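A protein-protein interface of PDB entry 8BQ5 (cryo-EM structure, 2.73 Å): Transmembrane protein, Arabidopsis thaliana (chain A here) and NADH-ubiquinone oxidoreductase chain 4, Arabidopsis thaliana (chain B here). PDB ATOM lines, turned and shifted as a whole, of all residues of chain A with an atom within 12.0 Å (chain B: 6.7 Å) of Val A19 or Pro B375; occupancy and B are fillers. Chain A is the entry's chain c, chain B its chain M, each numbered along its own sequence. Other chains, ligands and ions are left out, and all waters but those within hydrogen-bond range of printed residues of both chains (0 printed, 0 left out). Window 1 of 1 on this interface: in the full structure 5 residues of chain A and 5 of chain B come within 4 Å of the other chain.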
ATOM      1  N   GLY A  13      22.680 -16.760 -26.128  1.00  0.00           N
ATOM      2  CA  GLY A  13      22.638 -17.002 -27.558  1.00  0.00           C
ATOM      3  C   GLY A  13      23.992 -17.373 -28.131  1.00  0.00           C
ATOM      4  O   GLY A  13      24.474 -18.488 -27.932  1.00  0.00           O
ATOM      5  N   ASP A  14      24.604 -16.438 -28.854  1.00  0.00           N
ATOM      6  CA  ASP A  14      25.941 -16.623 -29.401  1.00  0.00           C
ATOM      7  C   ASP A  14      26.963 -15.678 -28.790  1.00  0.00           C
ATOM      8  O   ASP A  14      27.965 -16.132 -28.231  1.00  0.00           O
ATOM      9  CB  ASP A  14      25.912 -16.443 -30.926  1.00  0.00           C
ATOM     10  CG  ASP A  14      25.215 -17.584 -31.633  1.00  0.00           C
ATOM     11  OD1 ASP A  14      25.005 -18.640 -30.999  1.00  0.00           O
ATOM     12  OD2 ASP A  14      24.871 -17.426 -32.822  1.00  0.00           O
ATOM     13  N   PHE A  15      26.735 -14.366 -28.872  1.00  0.00           N
ATOM     14  CA  PHE A  15      27.674 -13.425 -28.273  1.00  0.00           C
ATOM     15  C   PHE A  15      27.539 -13.377 -26.758  1.00  0.00           C
ATOM     16  O   PHE A  15      28.514 -13.068 -26.065  1.00  0.00           O
ATOM     17  CB  PHE A  15      27.497 -12.029 -28.882  1.00  0.00           C
ATOM     18  CG  PHE A  15      26.242 -11.319 -28.451  1.00  0.00           C
ATOM     19  CD1 PHE A  15      26.213 -10.561 -27.289  1.00  0.00           C
ATOM     20  CD2 PHE A  15      25.096 -11.392 -29.221  1.00  0.00           C
ATOM     21  CE1 PHE A  15      25.063  -9.908 -26.899  1.00  0.00           C
ATOM     22  CE2 PHE A  15      23.945 -10.737 -28.836  1.00  0.00           C
ATOM     23  CZ  PHE A  15      23.929  -9.996 -27.674  1.00  0.00           C
ATOM     24  N   ARG A  16      26.353 -13.685 -26.227  1.00  0.00           N
ATOM     25  CA  ARG A  16      26.160 -13.666 -24.783  1.00  0.00           C
ATOM     26  C   ARG A  16      27.025 -14.696 -24.071  1.00  0.00           C
ATOM     27  O   ARG A  16      27.241 -14.575 -22.861  1.00  0.00           O
ATOM     28  CB  ARG A  16      24.684 -13.882 -24.450  1.00  0.00           C
ATOM     29  CG  ARG A  16      23.751 -12.970 -25.231  1.00  0.00           C
ATOM     30  CD  ARG A  16      22.346 -12.976 -24.665  1.00  0.00           C
ATOM     31  NE  ARG A  16      21.599 -14.160 -25.069  1.00  0.00           N
ATOM     32  CZ  ARG A  16      20.288 -14.191 -25.255  1.00  0.00           C
ATOM     33  NH1 ARG A  16      19.541 -13.111 -25.095  1.00  0.00           N
ATOM     34  NH2 ARG A  16      19.711 -15.333 -25.620  1.00  0.00           N
ATOM     35  N   ALA A  17      27.528 -15.700 -24.792  1.00  0.00           N
ATOM     36  CA  ALA A  17      28.484 -16.640 -24.224  1.00  0.00           C
ATOM     37  C   ALA A  17      29.846 -16.011 -23.970  1.00  0.00           C
ATOM     38  O   ALA A  17      30.637 -16.572 -23.204  1.00  0.00           O
ATOM     39  CB  ALA A  17      28.639 -17.852 -25.143  1.00  0.00           C
ATOM     40  N   LYS A  18      30.145 -14.872 -24.591  1.00  0.00           N
ATOM     41  CA  LYS A  18      31.376 -14.141 -24.332  1.00  0.00           C
ATOM     42  C   LYS A  18      31.154 -12.934 -23.432  1.00  0.00           C
ATOM     43  O   LYS A  18      32.028 -12.067 -23.346  1.00  0.00           O
ATOM     44  CB  LYS A  18      32.024 -13.704 -25.648  1.00  0.00           C
ATOM     45  CG  LYS A  18      32.032 -14.778 -26.725  1.00  0.00           C
ATOM     46  CD  LYS A  18      33.298 -14.721 -27.579  1.00  0.00           C
ATOM     47  CE  LYS A  18      33.794 -13.298 -27.798  1.00  0.00           C
ATOM     48  NZ  LYS A  18      33.162 -12.665 -28.988  1.00  0.00           N
ATOM     49  N   VAL A  19      30.009 -12.860 -22.760  1.00  0.00           N
ATOM     50  CA  VAL A  19      29.662 -11.732 -21.904  1.00  0.00           C
ATOM     51  C   VAL A  19      29.642 -12.217 -20.462  1.00  0.00           C
ATOM     52  O   VAL A  19      28.926 -13.170 -20.128  1.00  0.00           O
ATOM     53  CB  VAL A  19      28.311 -11.116 -22.297  1.00  0.00           C
ATOM     54  CG1 VAL A  19      27.836 -10.158 -21.219  1.00  0.00           C
ATOM     55  CG2 VAL A  19      28.420 -10.410 -23.637  1.00  0.00           C
ATOM     56  N   TRP A  20      30.420 -11.558 -19.613  1.00  0.00           N
ATOM     57  CA  TRP A  20      30.481 -11.874 -18.193  1.00  0.00           C
ATOM     58  C   TRP A  20      29.460 -11.037 -17.435  1.00  0.00           C
ATOM     59  O   TRP A  20      29.384  -9.820 -17.624  1.00  0.00           O
ATOM     60  CB  TRP A  20      31.887 -11.608 -17.655  1.00  0.00           C
ATOM     61  CG  TRP A  20      32.144 -12.121 -16.272  1.00  0.00           C
ATOM     62  CD1 TRP A  20      32.749 -13.295 -15.936  1.00  0.00           C
ATOM     63  CD2 TRP A  20      31.826 -11.466 -15.036  1.00  0.00           C
ATOM     64  NE1 TRP A  20      32.819 -13.417 -14.570  1.00  0.00           N
ATOM     65  CE2 TRP A  20      32.260 -12.308 -13.995  1.00  0.00           C
ATOM     66  CE3 TRP A  20      31.212 -10.252 -14.711  1.00  0.00           C
ATOM     67  CZ2 TRP A  20      32.102 -11.975 -12.651  1.00  0.00           C
ATOM     68  CZ3 TRP A  20      31.055  -9.925 -13.377  1.00  0.00           C
ATOM     69  CH2 TRP A  20      31.497 -10.784 -12.364  1.00  0.00           C
ATOM     70  N   SER A  21      28.674 -11.693 -16.583  1.00  0.00           N
ATOM     71  CA  SER A  21      27.751 -11.005 -15.694  1.00  0.00           C
ATOM     72  C   SER A  21      27.792 -11.676 -14.329  1.00  0.00           C
ATOM     73  O   SER A  21      28.189 -12.835 -14.196  1.00  0.00           O
ATOM     74  CB  SER A  21      26.317 -10.999 -16.238  1.00  0.00           C
ATOM     75  OG  SER A  21      25.841 -12.316 -16.445  1.00  0.00           O
ATOM     76  N   MET A  22      27.391 -10.922 -13.306  1.00  0.00           N
ATOM     77  CA  MET A  22      27.381 -11.469 -11.953  1.00  0.00           C
ATOM     78  C   MET A  22      26.223 -12.434 -11.757  1.00  0.00           C
ATOM     79  O   MET A  22      26.337 -13.407 -11.003  1.00  0.00           O
ATOM     80  CB  MET A  22      27.309 -10.339 -10.930  1.00  0.00           C
ATOM     81  CG  MET A  22      27.774  -9.000 -11.455  1.00  0.00           C
ATOM     82  SD  MET A  22      27.508  -7.684 -10.258  1.00  0.00           S
ATOM     83  CE  MET A  22      28.566  -8.241  -8.928  1.00  0.00           C
ATOM     84  N   THR A  23      25.100 -12.179 -12.421  1.00  0.00           N
ATOM     85  CA  THR A  23      23.917 -13.011 -12.265  1.00  0.00           C
ATOM     86  C   THR A  23      23.977 -14.278 -13.108  1.00  0.00           C
ATOM     87  O   THR A  23      23.128 -15.160 -12.939  1.00  0.00           O
ATOM     88  CB  THR A  23      22.672 -12.198 -12.618  1.00  0.00           C
ATOM     89  OG1 THR A  23      22.874 -10.840 -12.216  1.00  0.00           O
ATOM     90  CG2 THR A  23      21.465 -12.734 -11.883  1.00  0.00           C
ATOM     91  N   GLY A  24      24.958 -14.393 -14.000  1.00  0.00           N
ATOM     92  CA  GLY A  24      25.182 -15.606 -14.754  1.00  0.00           C
ATOM     93  C   GLY A  24      24.806 -15.538 -16.216  1.00  0.00           C
ATOM     94  O   GLY A  24      25.367 -16.298 -17.014  1.00  0.00           O
ATOM     95  N   GLY A  25      23.888 -14.656 -16.595  1.00  0.00           N
ATOM     96  CA  GLY A  25      23.463 -14.552 -17.968  1.00  0.00           C
ATOM     97  C   GLY A  25      22.340 -15.513 -18.299  1.00  0.00           C
ATOM     98  O   GLY A  25      21.759 -16.155 -17.420  1.00  0.00           O
ATOM     99  N   PRO A  26      22.013 -15.628 -19.583  1.00  0.00           N
ATOM    100  CA  PRO A  26      20.909 -16.505 -19.987  1.00  0.00           C
ATOM    101  C   PRO A  26      21.312 -17.970 -19.949  1.00  0.00           C
ATOM    102  O   PRO A  26      22.363 -18.360 -20.465  1.00  0.00           O
ATOM    103  CB  PRO A  26      20.601 -16.051 -21.418  1.00  0.00           C
ATOM    104  CG  PRO A  26      21.885 -15.470 -21.919  1.00  0.00           C
ATOM    105  CD  PRO A  26      22.694 -15.013 -20.735  1.00  0.00           C
ATOM    106  N   ASN A  27      20.452 -18.781 -19.329  1.00  0.00           N
ATOM    107  CA  ASN A  27      20.641 -20.230 -19.233  1.00  0.00           C
ATOM    108  C   ASN A  27      21.947 -20.576 -18.519  1.00  0.00           C
ATOM    109  O   ASN A  27      22.843 -21.205 -19.083  1.00  0.00           O
ATOM    110  CB  ASN A  27      20.590 -20.882 -20.617  1.00  0.00           C
ATOM    111  CG  ASN A  27      19.299 -20.593 -21.350  1.00  0.00           C
ATOM    112  OD1 ASN A  27      18.209 -20.843 -20.837  1.00  0.00           O
ATOM    113  ND2 ASN A  27      19.415 -20.060 -22.560  1.00  0.00           N
ATOM    114  N   CYS A  28      22.047 -20.168 -17.258  1.00  0.00           N
ATOM    115  CA  CYS A  28      23.240 -20.442 -16.469  1.00  0.00           C
ATOM    116  C   CYS A  28      23.114 -21.812 -15.813  1.00  0.00           C
ATOM    117  O   CYS A  28      22.184 -22.051 -15.033  1.00  0.00           O
ATOM    118  CB  CYS A  28      23.449 -19.355 -15.418  1.00  0.00           C
ATOM    119  SG  CYS A  28      25.053 -19.416 -14.595  1.00  0.00           S
ATOM    120  N   ARG A  29      24.042 -22.712 -16.133  1.00  0.00           N
ATOM    121  CA  ARG A  29      24.065 -24.070 -15.592  1.00  0.00           C
ATOM    122  C   ARG A  29      25.481 -24.419 -15.153  1.00  0.00           C
ATOM    123  O   ARG A  29      26.159 -25.228 -15.798  1.00  0.00           O
ATOM    124  CB  ARG A  29      23.567 -25.077 -16.630  1.00  0.00           C
ATOM    125  CG  ARG A  29      22.144 -24.859 -17.105  1.00  0.00           C
ATOM    126  CD  ARG A  29      21.137 -25.550 -16.205  1.00  0.00           C
ATOM    127  NE  ARG A  29      21.581 -26.877 -15.793  1.00  0.00           N
ATOM    128  CZ  ARG A  29      20.802 -27.779 -15.212  1.00  0.00           C
ATOM    129  NH1 ARG A  29      19.515 -27.550 -15.006  1.00  0.00           N
ATOM    130  NH2 ARG A  29      21.324 -28.942 -14.834  1.00  0.00           N
ATOM    131  N   LEU B 370      22.221  -1.978 -24.338  1.00  0.00           N
ATOM    132  CA  LEU B 370      23.554  -2.199 -23.796  1.00  0.00           C
ATOM    133  C   LEU B 370      23.562  -3.144 -22.603  1.00  0.00           C
ATOM    134  O   LEU B 370      24.644  -3.563 -22.176  1.00  0.00           O
ATOM    135  CB  LEU B 370      24.180  -0.862 -23.402  1.00  0.00           C
ATOM    136  CG  LEU B 370      24.660   0.002 -24.566  1.00  0.00           C
ATOM    137  CD1 LEU B 370      25.284   1.277 -24.049  1.00  0.00           C
ATOM    138  CD2 LEU B 370      25.643  -0.762 -25.430  1.00  0.00           C
ATOM    139  N   VAL B 371      22.396  -3.483 -22.050  1.00  0.00           N
ATOM    140  CA  VAL B 371      22.349  -4.413 -20.925  1.00  0.00           C
ATOM    141  C   VAL B 371      22.824  -5.797 -21.347  1.00  0.00           C
ATOM    142  O   VAL B 371      23.423  -6.527 -20.548  1.00  0.00           O
ATOM    143  CB  VAL B 371      20.929  -4.449 -20.320  1.00  0.00           C
ATOM    144  CG1 VAL B 371      19.907  -4.871 -21.361  1.00  0.00           C
ATOM    145  CG2 VAL B 371      20.880  -5.368 -19.112  1.00  0.00           C
ATOM    146  N   SER B 372      22.578  -6.180 -22.601  1.00  0.00           N
ATOM    147  CA  SER B 372      22.955  -7.507 -23.069  1.00  0.00           C
ATOM    148  C   SER B 372      24.420  -7.600 -23.475  1.00  0.00           C
ATOM    149  O   SER B 372      24.932  -8.712 -23.635  1.00  0.00           O
ATOM    150  CB  SER B 372      22.072  -7.922 -24.245  1.00  0.00           C
ATOM    151  OG  SER B 372      22.436  -7.224 -25.422  1.00  0.00           O
ATOM    152  N   THR B 373      25.103  -6.469 -23.647  1.00  0.00           N
ATOM    153  CA  THR B 373      26.515  -6.475 -24.001  1.00  0.00           C
ATOM    154  C   THR B 373      27.413  -5.859 -22.939  1.00  0.00           C
ATOM    155  O   THR B 373      28.593  -6.214 -22.877  1.00  0.00           O
ATOM    156  CB  THR B 373      26.740  -5.737 -25.329  1.00  0.00           C
ATOM    157  OG1 THR B 373      26.255  -4.393 -25.220  1.00  0.00           O
ATOM    158  CG2 THR B 373      26.012  -6.441 -26.456  1.00  0.00           C
ATOM    159  N   MET B 374      26.891  -4.958 -22.110  1.00  0.00           N
ATOM    160  CA  MET B 374      27.663  -4.317 -21.044  1.00  0.00           C
ATOM    161  C   MET B 374      26.896  -4.385 -19.727  1.00  0.00           C
ATOM    162  O   MET B 374      26.485  -3.358 -19.181  1.00  0.00           O
ATOM    163  CB  MET B 374      27.981  -2.869 -21.411  1.00  0.00           C
ATOM    164  CG  MET B 374      28.616  -2.693 -22.778  1.00  0.00           C
ATOM    165  SD  MET B 374      28.744  -0.966 -23.276  1.00  0.00           S
ATOM    166  CE  MET B 374      30.038  -0.390 -22.184  1.00  0.00           C
ATOM    167  N   PRO B 375      26.682  -5.589 -19.187  1.00  0.00           N
ATOM    168  CA  PRO B 375      25.925  -5.694 -17.929  1.00  0.00           C
ATOM    169  C   PRO B 375      26.597  -5.027 -16.740  1.00  0.00           C
ATOM    170  O   PRO B 375      25.898  -4.468 -15.885  1.00  0.00           O
ATOM    171  CB  PRO B 375      25.794  -7.210 -17.728  1.00  0.00           C
ATOM    172  CG  PRO B 375      26.933  -7.791 -18.480  1.00  0.00           C
ATOM    173  CD  PRO B 375      27.159  -6.900 -19.659  1.00  0.00           C
ATOM    174  N   ASN B 376      27.928  -5.067 -16.648  1.00  0.00           N
ATOM    175  CA  ASN B 376      28.600  -4.423 -15.523  1.00  0.00           C
ATOM    176  C   ASN B 376      28.470  -2.907 -15.603  1.00  0.00           C
ATOM    177  O   ASN B 376      28.206  -2.243 -14.595  1.00  0.00           O
ATOM    178  CB  ASN B 376      30.069  -4.842 -15.472  1.00  0.00           C
ATOM    179  CG  ASN B 376      30.284  -6.095 -14.649  1.00  0.00           C
ATOM    180  OD1 ASN B 376      29.395  -6.533 -13.920  1.00  0.00           O
ATOM    181  ND2 ASN B 376      31.467  -6.682 -14.766  1.00  0.00           N
ATOM    182  N   PHE B 377      28.650  -2.341 -16.798  1.00  0.00           N
ATOM    183  CA  PHE B 377      28.405  -0.915 -16.975  1.00  0.00           C
ATOM    184  C   PHE B 377      26.942  -0.580 -16.713  1.00  0.00           C
ATOM    185  O   PHE B 377      26.633   0.453 -16.110  1.00  0.00           O
ATOM    186  CB  PHE B 377      28.817  -0.473 -18.381  1.00  0.00           C
ATOM    187  CG  PHE B 377      28.247   0.857 -18.787  1.00  0.00           C
ATOM    188  CD1 PHE B 377      28.889   2.034 -18.441  1.00  0.00           C
ATOM    189  CD2 PHE B 377      27.072   0.931 -19.515  1.00  0.00           C
ATOM    190  CE1 PHE B 377      28.366   3.258 -18.808  1.00  0.00           C
ATOM    191  CE2 PHE B 377      26.544   2.152 -19.883  1.00  0.00           C
ATOM    192  CZ  PHE B 377      27.193   3.316 -19.530  1.00  0.00           C
ATOM    193  N   SER B 378      26.031  -1.445 -17.162  1.00  0.00           N
ATOM    194  CA  SER B 378      24.604  -1.197 -16.976  1.00  0.00           C
ATOM    195  C   SER B 378      24.227  -1.182 -15.499  1.00  0.00           C
ATOM    196  O   SER B 378      23.399  -0.370 -15.071  1.00  0.00           O
ATOM    197  CB  SER B 378      23.792  -2.252 -17.723  1.00  0.00           C
ATOM    198  OG  SER B 378      23.995  -2.151 -19.120  1.00  0.00           O
ATOM    199  N   THR B 379      24.801  -2.092 -14.712  1.00  0.00           N
ATOM    200  CA  THR B 379      24.513  -2.126 -13.281  1.00  0.00           C
ATOM    201  C   THR B 379      25.030  -0.873 -12.584  1.00  0.00           C
ATOM    202  O   THR B 379      24.344  -0.292 -11.735  1.00  0.00           O
ATOM    203  CB  THR B 379      25.117  -3.384 -12.657  1.00  0.00           C
ATOM    204  OG1 THR B 379      24.449  -4.540 -13.174  1.00  0.00           O
ATOM    205  CG2 THR B 379      24.973  -3.358 -11.145  1.00  0.00           C
ATOM    206  N   ILE B 380      26.246  -0.442 -12.928  1.00  0.00           N
ATOM    207  CA  ILE B 380      26.814   0.760 -12.324  1.00  0.00           C
ATOM    208  C   ILE B 380      26.081   2.002 -12.814  1.00  0.00           C
ATOM    209  O   ILE B 380      25.840   2.942 -12.048  1.00  0.00           O
ATOM    210  CB  ILE B 380      28.329   0.828 -12.600  1.00  0.00           C
ATOM    211  CG1 ILE B 380      29.070  -0.117 -11.653  1.00  0.00           C
ATOM    212  CG2 ILE B 380      28.853   2.246 -12.449  1.00  0.00           C
ATOM    213  CD1 ILE B 380      30.496  -0.396 -12.048  1.00  0.00           C
ATOM    214  N   ASP B 451      32.670  -4.371 -22.141  1.00  0.00           N
ATOM    215  CA  ASP B 451      32.297  -3.924 -20.808  1.00  0.00           C
ATOM    216  C   ASP B 451      33.486  -3.237 -20.133  1.00  0.00           C
ATOM    217  O   ASP B 451      34.569  -3.091 -20.709  1.00  0.00           O
ATOM    218  CB  ASP B 451      31.785  -5.100 -19.980  1.00  0.00           C
ATOM    219  CG  ASP B 451      30.672  -4.709 -19.036  1.00  0.00           C
ATOM    220  OD1 ASP B 451      30.555  -3.508 -18.720  1.00  0.00           O
ATOM    221  OD2 ASP B 451      29.910  -5.601 -18.610  1.00  0.00           O
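Phe A15 touches Ser B372 (CE1 to O, 3.5 Å). CE1 of Phe A15 touches CG2 of Thr B373 (3.6 Å). Ser B372 touches Val A19. CG1 of Val A19 touches CD of Pro B375 (3.7 Å). Pro B375 touches Trp A20. Trp A20 touches Asn B376. Ser A21 touches Pro B375 (CB to CG, 3.96 Å). Met A22 touches Asn B376 (CG to OD1, 3.8 Å).
The side-chain hydroxyl (OG1) of Thr B379 sits at hydrogen-bond distance from the backbone carbonyl oxygen (O) of Pro B375. N of Asn B376 is in hydrogen-bond range of OD2 of Asp B451 (2.8 Å). OG of Ser A21 is in hydrogen-bond range of N of Gly A24, at 3.3 Å. The backbone NH (N) of Gly A25 sits at hydrogen-bond distance from the side-chain hydroxyl (OG) of Ser A21 (3.1 Å).
Gly A13 touches none of the printed residues of chain B. Of the printed residues of chain B, Phe A15 touches Ser B372 and Thr B373. Val A19 touches just these residues of chain B: Ser B372 (3.9 Å) and Pro B375 (3.7 Å). Of the printed residues of chain B, Trp A20 touches Pro B375 and Asn B376. Of the printed residues of chain B, Ser A21 touches Pro B375 (3.96 Å). Val B371 touches none of the printed residues of chain A. Ser B372 touches just these residues of chain A: Phe A15 and Val A19. No residue of chain A comes within 4 Å of Met B374. Pro B375 touches just these residues of chain A: Val A19, Trp A20 and Ser A21. Asn B376 touches just these residues of chain A: Trp A20 (3.6 Å) and Met A22 (3.8 Å). No residue of chain A comes within 4 Å of Thr B379. Ile B380 touches none of the printed residues of chain A. The nearest printed residue of chain B that does not touch Ser A21 is Asn B376 (5.1 Å).
Of the 17 printed residues of chain A, 5 touch a printed residue of chain B. Hydrophobic or aromatic side chains of chain A within 4 Å of the printed part of chain B: Phe A15, Val A19, Trp A20 and Met A22. Hydrophobic or aromatic side chains of chain B that line the printed part of chain A: Pro B375. Along chain B the printed residues that touch a printed residue of chain A span positions 372 to 376. Among the printed residues, 8 pairs touch across the chains. Among the printed residues, no Asp or Glu carboxylate lies within 4 Å of a Lys or Arg side-chain nitrogen of the other chain.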
